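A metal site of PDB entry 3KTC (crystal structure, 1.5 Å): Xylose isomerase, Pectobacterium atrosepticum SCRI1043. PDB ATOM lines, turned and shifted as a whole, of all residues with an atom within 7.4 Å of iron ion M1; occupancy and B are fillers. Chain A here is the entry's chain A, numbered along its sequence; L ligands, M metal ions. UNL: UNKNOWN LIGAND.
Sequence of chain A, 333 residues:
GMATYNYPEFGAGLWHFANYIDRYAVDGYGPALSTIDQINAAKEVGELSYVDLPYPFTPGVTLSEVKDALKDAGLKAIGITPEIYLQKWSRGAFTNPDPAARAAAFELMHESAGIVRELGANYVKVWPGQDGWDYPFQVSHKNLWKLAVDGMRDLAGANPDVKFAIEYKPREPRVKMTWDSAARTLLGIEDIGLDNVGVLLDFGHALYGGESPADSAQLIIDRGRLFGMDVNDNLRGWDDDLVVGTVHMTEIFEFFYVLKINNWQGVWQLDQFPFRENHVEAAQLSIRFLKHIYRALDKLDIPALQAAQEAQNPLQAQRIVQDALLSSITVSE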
ATOM      1  N   TRP A  15      -8.453 -10.372  35.885  1.00  0.00           N
ATOM      2  CA  TRP A  15      -8.156  -9.020  35.442  1.00  0.00           C
ATOM      3  C   TRP A  15      -9.367  -8.264  34.898  1.00  0.00           C
ATOM      4  O   TRP A  15      -9.303  -7.058  34.760  1.00  0.00           O
ATOM      5  CB  TRP A  15      -7.040  -9.029  34.399  1.00  0.00           C
ATOM      6  CG  TRP A  15      -7.403  -9.836  33.183  1.00  0.00           C
ATOM      7  CD1 TRP A  15      -8.061  -9.393  32.081  1.00  0.00           C
ATOM      8  CD2 TRP A  15      -7.158 -11.238  32.975  1.00  0.00           C
ATOM      9  NE1 TRP A  15      -8.238 -10.415  31.203  1.00  0.00           N
ATOM     10  CE2 TRP A  15      -7.701 -11.565  31.715  1.00  0.00           C
ATOM     11  CE3 TRP A  15      -6.549 -12.244  33.737  1.00  0.00           C
ATOM     12  CZ2 TRP A  15      -7.640 -12.852  31.190  1.00  0.00           C
ATOM     13  CZ3 TRP A  15      -6.500 -13.515  33.225  1.00  0.00           C
ATOM     14  CH2 TRP A  15      -7.036 -13.814  31.958  1.00  0.00           C
ATOM     15  N   LYS A 125      -2.306 -20.989  31.372  1.00  0.00           N
ATOM     16  CA  LYS A 125      -2.688 -20.162  30.223  1.00  0.00           C
ATOM     17  C   LYS A 125      -1.439 -19.358  29.824  1.00  0.00           C
ATOM     18  O   LYS A 125      -0.995 -18.472  30.554  1.00  0.00           O
ATOM     19  CB  LYS A 125      -3.827 -19.256  30.638  1.00  0.00           C
ATOM     20  CG  LYS A 125      -4.706 -18.792  29.516  1.00  0.00           C
ATOM     21  CD  LYS A 125      -4.112 -17.781  28.610  1.00  0.00           C
ATOM     22  CE  LYS A 125      -3.778 -16.441  29.297  1.00  0.00           C
ATOM     23  NZ  LYS A 125      -4.907 -15.847  30.065  1.00  0.00           N
ATOM     24  N   TRP A 127       0.389 -16.834  27.535  1.00  0.00           N
ATOM     25  CA  TRP A 127       0.235 -15.703  26.607  1.00  0.00           C
ATOM     26  C   TRP A 127       1.516 -14.906  26.612  1.00  0.00           C
ATOM     27  O   TRP A 127       1.724 -14.078  27.460  1.00  0.00           O
ATOM     28  CB  TRP A 127      -0.926 -14.792  26.985  1.00  0.00           C
ATOM     29  CG  TRP A 127      -1.012 -13.659  26.039  1.00  0.00           C
ATOM     30  CD1 TRP A 127      -1.352 -13.708  24.715  1.00  0.00           C
ATOM     31  CD2 TRP A 127      -0.707 -12.291  26.318  1.00  0.00           C
ATOM     32  NE1 TRP A 127      -1.271 -12.456  24.162  1.00  0.00           N
ATOM     33  CE2 TRP A 127      -0.853 -11.568  25.121  1.00  0.00           C
ATOM     34  CE3 TRP A 127      -0.272 -11.613  27.460  1.00  0.00           C
ATOM     35  CZ2 TRP A 127      -0.622 -10.193  25.041  1.00  0.00           C
ATOM     36  CZ3 TRP A 127      -0.069 -10.261  27.392  1.00  0.00           C
ATOM     37  CH2 TRP A 127      -0.240  -9.564  26.198  1.00  0.00           C
ATOM     38  N   GLU A 167      -2.507 -18.912  24.194  1.00  0.00           N
ATOM     39  CA  GLU A 167      -3.451 -17.907  23.726  1.00  0.00           C
ATOM     40  C   GLU A 167      -2.844 -17.113  22.600  1.00  0.00           C
ATOM     41  O   GLU A 167      -2.060 -16.197  22.828  1.00  0.00           O
ATOM     42  CB  GLU A 167      -3.906 -16.980  24.864  1.00  0.00           C
ATOM     43  CG  GLU A 167      -4.923 -16.006  24.379  1.00  0.00           C
ATOM     44  CD  GLU A 167      -5.534 -15.225  25.475  1.00  0.00           C
ATOM     45  OE1 GLU A 167      -4.983 -15.170  26.585  1.00  0.00           O
ATOM     46  OE2 GLU A 167      -6.564 -14.603  25.211  1.00  0.00           O
ATOM     47  N   TYR A 168      -3.154 -17.490  21.382  1.00  0.00           N
ATOM     48  CA  TYR A 168      -2.619 -16.729  20.273  1.00  0.00           C
ATOM     49  C   TYR A 168      -3.241 -15.344  20.193  1.00  0.00           C
ATOM     50  O   TYR A 168      -4.327 -15.107  20.673  1.00  0.00           O
ATOM     51  CB  TYR A 168      -2.801 -17.473  18.958  1.00  0.00           C
ATOM     52  CG  TYR A 168      -4.193 -17.607  18.410  1.00  0.00           C
ATOM     53  CD1 TYR A 168      -4.754 -16.596  17.626  1.00  0.00           C
ATOM     54  CD2 TYR A 168      -4.942 -18.745  18.620  1.00  0.00           C
ATOM     55  CE1 TYR A 168      -6.024 -16.706  17.064  1.00  0.00           C
ATOM     56  CE2 TYR A 168      -6.206 -18.875  18.065  1.00  0.00           C
ATOM     57  CZ  TYR A 168      -6.752 -17.861  17.304  1.00  0.00           C
ATOM     58  OH  TYR A 168      -8.000 -18.065  16.723  1.00  0.00           O
ATOM     59  N   LYS A 169      -2.505 -14.424  19.579  1.00  0.00           N
ATOM     60  CA  LYS A 169      -2.919 -13.052  19.451  1.00  0.00           C
ATOM     61  C   LYS A 169      -2.115 -12.430  18.312  1.00  0.00           C
ATOM     62  O   LYS A 169      -0.932 -12.655  18.242  1.00  0.00           O
ATOM     63  CB  LYS A 169      -2.675 -12.273  20.747  1.00  0.00           C
ATOM     64  CG  LYS A 169      -3.379 -10.931  20.802  1.00  0.00           C
ATOM     65  CD  LYS A 169      -2.932 -10.146  22.000  1.00  0.00           C
ATOM     66  CE  LYS A 169      -3.655  -8.825  22.078  1.00  0.00           C
ATOM     67  NZ  LYS A 169      -3.129  -7.981  23.201  1.00  0.00           N
ATOM     68  N   LEU A 200      -5.870 -21.657  23.684  1.00  0.00           N
ATOM     69  CA  LEU A 200      -6.904 -20.816  24.302  1.00  0.00           C
ATOM     70  C   LEU A 200      -7.344 -19.880  23.160  1.00  0.00           C
ATOM     71  O   LEU A 200      -6.602 -19.006  22.742  1.00  0.00           O
ATOM     72  CB  LEU A 200      -6.339 -20.039  25.484  1.00  0.00           C
ATOM     73  CG  LEU A 200      -7.310 -19.361  26.462  1.00  0.00           C
ATOM     74  CD1 LEU A 200      -8.274 -18.414  25.751  1.00  0.00           C
ATOM     75  CD2 LEU A 200      -8.050 -20.398  27.313  1.00  0.00           C
ATOM     76  N   LEU A 201      -8.548 -20.098  22.645  1.00  0.00           N
ATOM     77  CA  LEU A 201      -9.061 -19.330  21.486  1.00  0.00           C
ATOM     78  C   LEU A 201      -9.843 -18.145  22.009  1.00  0.00           C
ATOM     79  O   LEU A 201     -10.896 -18.327  22.611  1.00  0.00           O
ATOM     80  CB  LEU A 201      -9.963 -20.228  20.622  1.00  0.00           C
ATOM     81  CG  LEU A 201     -10.299 -19.764  19.208  1.00  0.00           C
ATOM     82  CD1 LEU A 201     -11.313 -20.748  18.612  1.00  0.00           C
ATOM     83  CD2 LEU A 201     -10.798 -18.334  19.076  1.00  0.00           C
ATOM     84  N   ASP A 202      -9.302 -16.957  21.826  1.00  0.00           N
ATOM     85  CA  ASP A 202      -9.949 -15.708  22.220  1.00  0.00           C
ATOM     86  C   ASP A 202     -10.685 -15.239  20.987  1.00  0.00           C
ATOM     87  O   ASP A 202     -10.077 -14.940  19.948  1.00  0.00           O
ATOM     88  CB  ASP A 202      -8.904 -14.719  22.735  1.00  0.00           C
ATOM     89  CG  ASP A 202      -9.499 -13.408  23.205  1.00  0.00           C
ATOM     90  OD1 ASP A 202     -10.283 -12.795  22.452  1.00  0.00           O
ATOM     91  OD2 ASP A 202      -9.119 -12.960  24.310  1.00  0.00           O
ATOM     92  N   PHE A 203     -12.007 -15.209  21.087  1.00  0.00           N
ATOM     93  CA  PHE A 203     -12.850 -14.785  19.963  1.00  0.00           C
ATOM     94  C   PHE A 203     -12.396 -13.448  19.387  1.00  0.00           C
ATOM     95  O   PHE A 203     -12.342 -13.270  18.162  1.00  0.00           O
ATOM     96  CB  PHE A 203     -14.295 -14.689  20.421  1.00  0.00           C
ATOM     97  CG  PHE A 203     -15.208 -14.028  19.424  1.00  0.00           C
ATOM     98  CD1 PHE A 203     -15.856 -14.783  18.463  1.00  0.00           C
ATOM     99  CD2 PHE A 203     -15.426 -12.640  19.438  1.00  0.00           C
ATOM    100  CE1 PHE A 203     -16.706 -14.186  17.552  1.00  0.00           C
ATOM    101  CE2 PHE A 203     -16.288 -12.063  18.520  1.00  0.00           C
ATOM    102  CZ  PHE A 203     -16.888 -12.850  17.557  1.00  0.00           C
ATOM    103  N   GLY A 204     -12.121 -12.479  20.259  1.00  0.00           N
ATOM    104  CA  GLY A 204     -11.707 -11.160  19.829  1.00  0.00           C
ATOM    105  C   GLY A 204     -10.383 -11.169  19.075  1.00  0.00           C
ATOM    106  O   GLY A 204     -10.208 -10.448  18.094  1.00  0.00           O
ATOM    107  N   HIS A 205      -9.451 -11.996  19.529  1.00  0.00           N
ATOM    108  CA  HIS A 205      -8.153 -12.116  18.856  1.00  0.00           C
ATOM    109  C   HIS A 205      -8.334 -12.678  17.475  1.00  0.00           C
ATOM    110  O   HIS A 205      -7.743 -12.169  16.497  1.00  0.00           O
ATOM    111  CB  HIS A 205      -7.190 -12.986  19.660  1.00  0.00           C
ATOM    112  CG  HIS A 205      -6.830 -12.410  20.999  1.00  0.00           C
ATOM    113  ND1 HIS A 205      -5.906 -13.013  21.821  1.00  0.00           N
ATOM    114  CD2 HIS A 205      -7.244 -11.283  21.637  1.00  0.00           C
ATOM    115  CE1 HIS A 205      -5.790 -12.298  22.929  1.00  0.00           C
ATOM    116  NE2 HIS A 205      -6.611 -11.258  22.859  1.00  0.00           N
ATOM    117  N   MET A 229     -11.682 -21.166  25.831  1.00  0.00           N
ATOM    118  CA  MET A 229     -12.076 -20.025  25.031  1.00  0.00           C
ATOM    119  C   MET A 229     -12.051 -18.784  25.897  1.00  0.00           C
ATOM    120  O   MET A 229     -12.100 -18.870  27.116  1.00  0.00           O
ATOM    121  CB  MET A 229     -13.539 -20.155  24.563  1.00  0.00           C
ATOM    122  CG  MET A 229     -14.561 -19.402  25.582  1.00  0.00           C
ATOM    123  SD  MET A 229     -16.111 -19.408  25.240  1.00  0.00           S
ATOM    124  CE  MET A 229     -16.591 -21.325  25.506  1.00  0.00           C
ATOM    125  N   ASP A 230     -12.064 -17.620  25.254  1.00  0.00           N
ATOM    126  CA  ASP A 230     -12.244 -16.285  25.868  1.00  0.00           C
ATOM    127  C   ASP A 230     -13.233 -15.575  24.915  1.00  0.00           C
ATOM    128  O   ASP A 230     -13.103 -15.717  23.696  1.00  0.00           O
ATOM    129  CB  ASP A 230     -10.914 -15.435  25.835  1.00  0.00           C
ATOM    130  CG  ASP A 230     -10.063 -15.562  27.094  1.00  0.00           C
ATOM    131  OD1 ASP A 230     -10.577 -15.970  28.155  1.00  0.00           O
ATOM    132  OD2 ASP A 230      -8.869 -15.185  27.037  1.00  0.00           O
ATOM    133  N   VAL A 231     -14.186 -14.777  25.434  1.00  0.00           N
ATOM    134  CA  VAL A 231     -15.023 -13.938  24.570  1.00  0.00           C
ATOM    135  C   VAL A 231     -14.980 -12.491  25.025  1.00  0.00           C
ATOM    136  O   VAL A 231     -14.661 -12.191  26.162  1.00  0.00           O
ATOM    137  CB  VAL A 231     -16.457 -14.442  24.434  1.00  0.00           C
ATOM    138  CG1 VAL A 231     -16.409 -15.872  23.832  1.00  0.00           C
ATOM    139  CG2 VAL A 231     -17.188 -14.415  25.776  1.00  0.00           C
ATOM    140  N   ASN A 232     -15.343 -11.628  24.071  1.00  0.00           N
ATOM    141  CA  ASN A 232     -15.277 -10.166  24.155  1.00  0.00           C
ATOM    142  C   ASN A 232     -15.691  -9.690  22.764  1.00  0.00           C
ATOM    143  O   ASN A 232     -16.084 -10.489  21.922  1.00  0.00           O
ATOM    144  CB  ASN A 232     -13.869  -9.662  24.519  1.00  0.00           C
ATOM    145  CG  ASN A 232     -12.804 -10.228  23.644  1.00  0.00           C
ATOM    146  OD1 ASN A 232     -12.696  -9.869  22.472  1.00  0.00           O
ATOM    147  ND2 ASN A 232     -12.014 -11.148  24.193  1.00  0.00           N
ATOM    148  N   ASP A 239      -7.406  -5.339  19.626  1.00  0.00           N
ATOM    149  CA  ASP A 239      -7.949  -6.113  20.759  1.00  0.00           C
ATOM    150  C   ASP A 239      -8.670  -5.175  21.721  1.00  0.00           C
ATOM    151  O   ASP A 239      -8.204  -4.899  22.842  1.00  0.00           O
ATOM    152  CB  ASP A 239      -6.806  -6.833  21.470  1.00  0.00           C
ATOM    153  CG  ASP A 239      -7.277  -7.859  22.460  1.00  0.00           C
ATOM    154  OD1 ASP A 239      -8.388  -8.406  22.255  1.00  0.00           O
ATOM    155  OD2 ASP A 239      -6.547  -8.136  23.452  1.00  0.00           O
ATOM    156  N   ASP A 241     -11.323  -5.456  23.491  1.00  0.00           N
ATOM    157  CA  ASP A 241     -11.743  -6.097  24.747  1.00  0.00           C
ATOM    158  C   ASP A 241     -12.997  -5.472  25.330  1.00  0.00           C
ATOM    159  O   ASP A 241     -13.117  -5.295  26.530  1.00  0.00           O
ATOM    160  CB  ASP A 241     -10.591  -6.088  25.762  1.00  0.00           C
ATOM    161  CG  ASP A 241      -9.520  -7.093  25.436  1.00  0.00           C
ATOM    162  OD1 ASP A 241      -9.842  -8.178  24.930  1.00  0.00           O
ATOM    163  OD2 ASP A 241      -8.354  -6.810  25.764  1.00  0.00           O
ATOM    164  N   GLN A 269     -16.099 -18.162  29.010  1.00  0.00           N
ATOM    165  CA  GLN A 269     -15.158 -17.332  29.722  1.00  0.00           C
ATOM    166  C   GLN A 269     -14.983 -15.942  29.125  1.00  0.00           C
ATOM    167  O   GLN A 269     -14.693 -15.794  27.937  1.00  0.00           O
ATOM    168  CB  GLN A 269     -13.825 -18.056  29.717  1.00  0.00           C
ATOM    169  CG  GLN A 269     -12.633 -17.377  30.421  1.00  0.00           C
ATOM    170  CD  GLN A 269     -12.556 -17.630  31.909  1.00  0.00           C
ATOM    171  OE1 GLN A 269     -13.356 -18.372  32.467  1.00  0.00           O
ATOM    172  NE2 GLN A 269     -11.587 -17.002  32.560  1.00  0.00           N
ATOM    173  N   LEU A 270     -15.103 -14.928  29.976  1.00  0.00           N
ATOM    174  CA  LEU A 270     -14.967 -13.543  29.532  1.00  0.00           C
ATOM    175  C   LEU A 270     -13.527 -13.072  29.669  1.00  0.00           C
ATOM    176  O   LEU A 270     -12.904 -13.293  30.707  1.00  0.00           O
ATOM    177  CB  LEU A 270     -15.811 -12.639  30.426  1.00  0.00           C
ATOM    178  CG  LEU A 270     -17.307 -12.929  30.575  1.00  0.00           C
ATOM    179  CD1 LEU A 270     -17.929 -11.959  31.579  1.00  0.00           C
ATOM    180  CD2 LEU A 270     -17.934 -12.814  29.205  1.00  0.00           C
ATOM    181  N   ASP A 271     -12.987 -12.442  28.632  1.00  0.00           N
ATOM    182  CA  ASP A 271     -11.705 -11.745  28.741  1.00  0.00           C
ATOM    183  C   ASP A 271     -11.960 -10.345  28.201  1.00  0.00           C
ATOM    184  O   ASP A 271     -11.877 -10.098  26.983  1.00  0.00           O
ATOM    185  CB  ASP A 271     -10.628 -12.464  27.937  1.00  0.00           C
ATOM    186  CG  ASP A 271      -9.313 -11.729  27.935  1.00  0.00           C
ATOM    187  OD1 ASP A 271      -9.185 -10.711  28.634  1.00  0.00           O
ATOM    188  OD2 ASP A 271      -8.396 -12.156  27.233  1.00  0.00           O
ATOM    189  N   GLN A 272     -12.259  -9.431  29.130  1.00  0.00           N
ATOM    190  CA  GLN A 272     -12.705  -8.076  28.788  1.00  0.00           C
ATOM    191  C   GLN A 272     -12.026  -7.105  29.712  1.00  0.00           C
ATOM    192  O   GLN A 272     -11.707  -7.459  30.844  1.00  0.00           O
ATOM    193  CB  GLN A 272     -14.230  -7.992  28.935  1.00  0.00           C
ATOM    194  CG  GLN A 272     -14.934  -8.913  27.937  1.00  0.00           C
ATOM    195  CD  GLN A 272     -16.411  -9.144  28.126  1.00  0.00           C
ATOM    196  OE1 GLN A 272     -17.058  -9.593  27.168  1.00  0.00           O
ATOM    197  NE2 GLN A 272     -16.987  -8.846  29.301  1.00  0.00           N
ATOM    198  N   PHE A 273     -11.832  -5.891  29.225  1.00  0.00           N
ATOM    199  CA  PHE A 273     -11.177  -4.813  29.973  1.00  0.00           C
ATOM    200  C   PHE A 273     -12.089  -3.592  30.000  1.00  0.00           C
ATOM    201  O   PHE A 273     -12.016  -2.749  29.122  1.00  0.00           O
ATOM    202  CB  PHE A 273      -9.860  -4.392  29.289  1.00  0.00           C
ATOM    203  CG  PHE A 273      -8.678  -5.331  29.553  1.00  0.00           C
ATOM    204  CD1 PHE A 273      -8.642  -6.607  29.051  1.00  0.00           C
ATOM    205  CD2 PHE A 273      -7.564  -4.885  30.268  1.00  0.00           C
ATOM    206  CE1 PHE A 273      -7.542  -7.441  29.287  1.00  0.00           C
ATOM    207  CE2 PHE A 273      -6.481  -5.707  30.497  1.00  0.00           C
ATOM    208  CZ  PHE A 273      -6.471  -6.984  30.011  1.00  0.00           C
HETATM  209  O1  UNL L   1      -4.476 -11.474  26.330  1.00  0.00           O
HETATM  210  O2  UNL L   1      -4.432  -9.962  25.041  1.00  0.00           O
HETATM  211  O3  UNL L   1      -6.146 -11.667  25.859  1.00  0.00           O
HETATM  212  O4  UNL L   1      -5.757 -13.240  27.918  1.00  0.00           O
HETATM  213  O5  UNL L   1      -6.047 -10.439  28.364  1.00  0.00           O
HETATM  214  O6  UNL L   1      -4.027 -12.969  30.049  1.00  0.00           O
HETATM  215  O7  UNL L   1      -3.193 -11.462  32.154  1.00  0.00           O
HETATM  216  O8  UNL L   1      -3.920  -9.787  32.657  1.00  0.00           O
HETATM  217  O9  UNL L   1      -3.270  -9.155  31.227  1.00  0.00           O
HETATM  218 FE    FE M   1      -7.984 -13.529  26.050  1.00  0.00          FE
HETATM  219 FE    FE M   2      -8.070  -9.496  24.249  1.00  0.00          FE
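Of the 23 residues printed, 4 come within 4 Å of iron ion M1. Along chain A the residues within 4 Å of iron ion M1 span positions 167 to 271.
Iron ion M1 is bound by OD2 of Asp 271, OE2 of Glu 167, OD2 of Asp 230 and OD2 of Asp 202. Slightly farther from iron ion M1 lies an oxygen (O3) of the ligand (2.6 Å).
The backbone carbonyl oxygen (O) of Asp 230 sits at hydrogen-bond distance from the backbone NH (N) of Phe 203 (2.9 Å). The side-chain carboxylate (OD1) of Asp 202 is in hydrogen-bond range of the backbone NH (N) of His 205 (3.1 Å). The backbone carbonyl oxygen (O) of Val 231 is in hydrogen-bond range of the backbone NH (N) of Asp 271. The side-chain amide nitrogen (ND2) of Asn 232 is in hydrogen-bond range of the side-chain carboxylate (OD1) of Asp 202, 3.0 Å away. The backbone carbonyl oxygen (O) of Asp 271 lies within hydrogen-bond range of the side-chain amide nitrogen (ND2) of Asn 232 (3.0 Å). OD1 of Asp 202 lies within hydrogen-bond range of N of Gly 204, at 2.9 Å. The backbone NH (N) of Asp 230 lies within hydrogen-bond range of the backbone carbonyl oxygen (O) of Leu 201, at 3.0 Å. OE1 of Glu 167 lies within salt-bridge range of NZ of Lys 125, 3.5 Å away.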
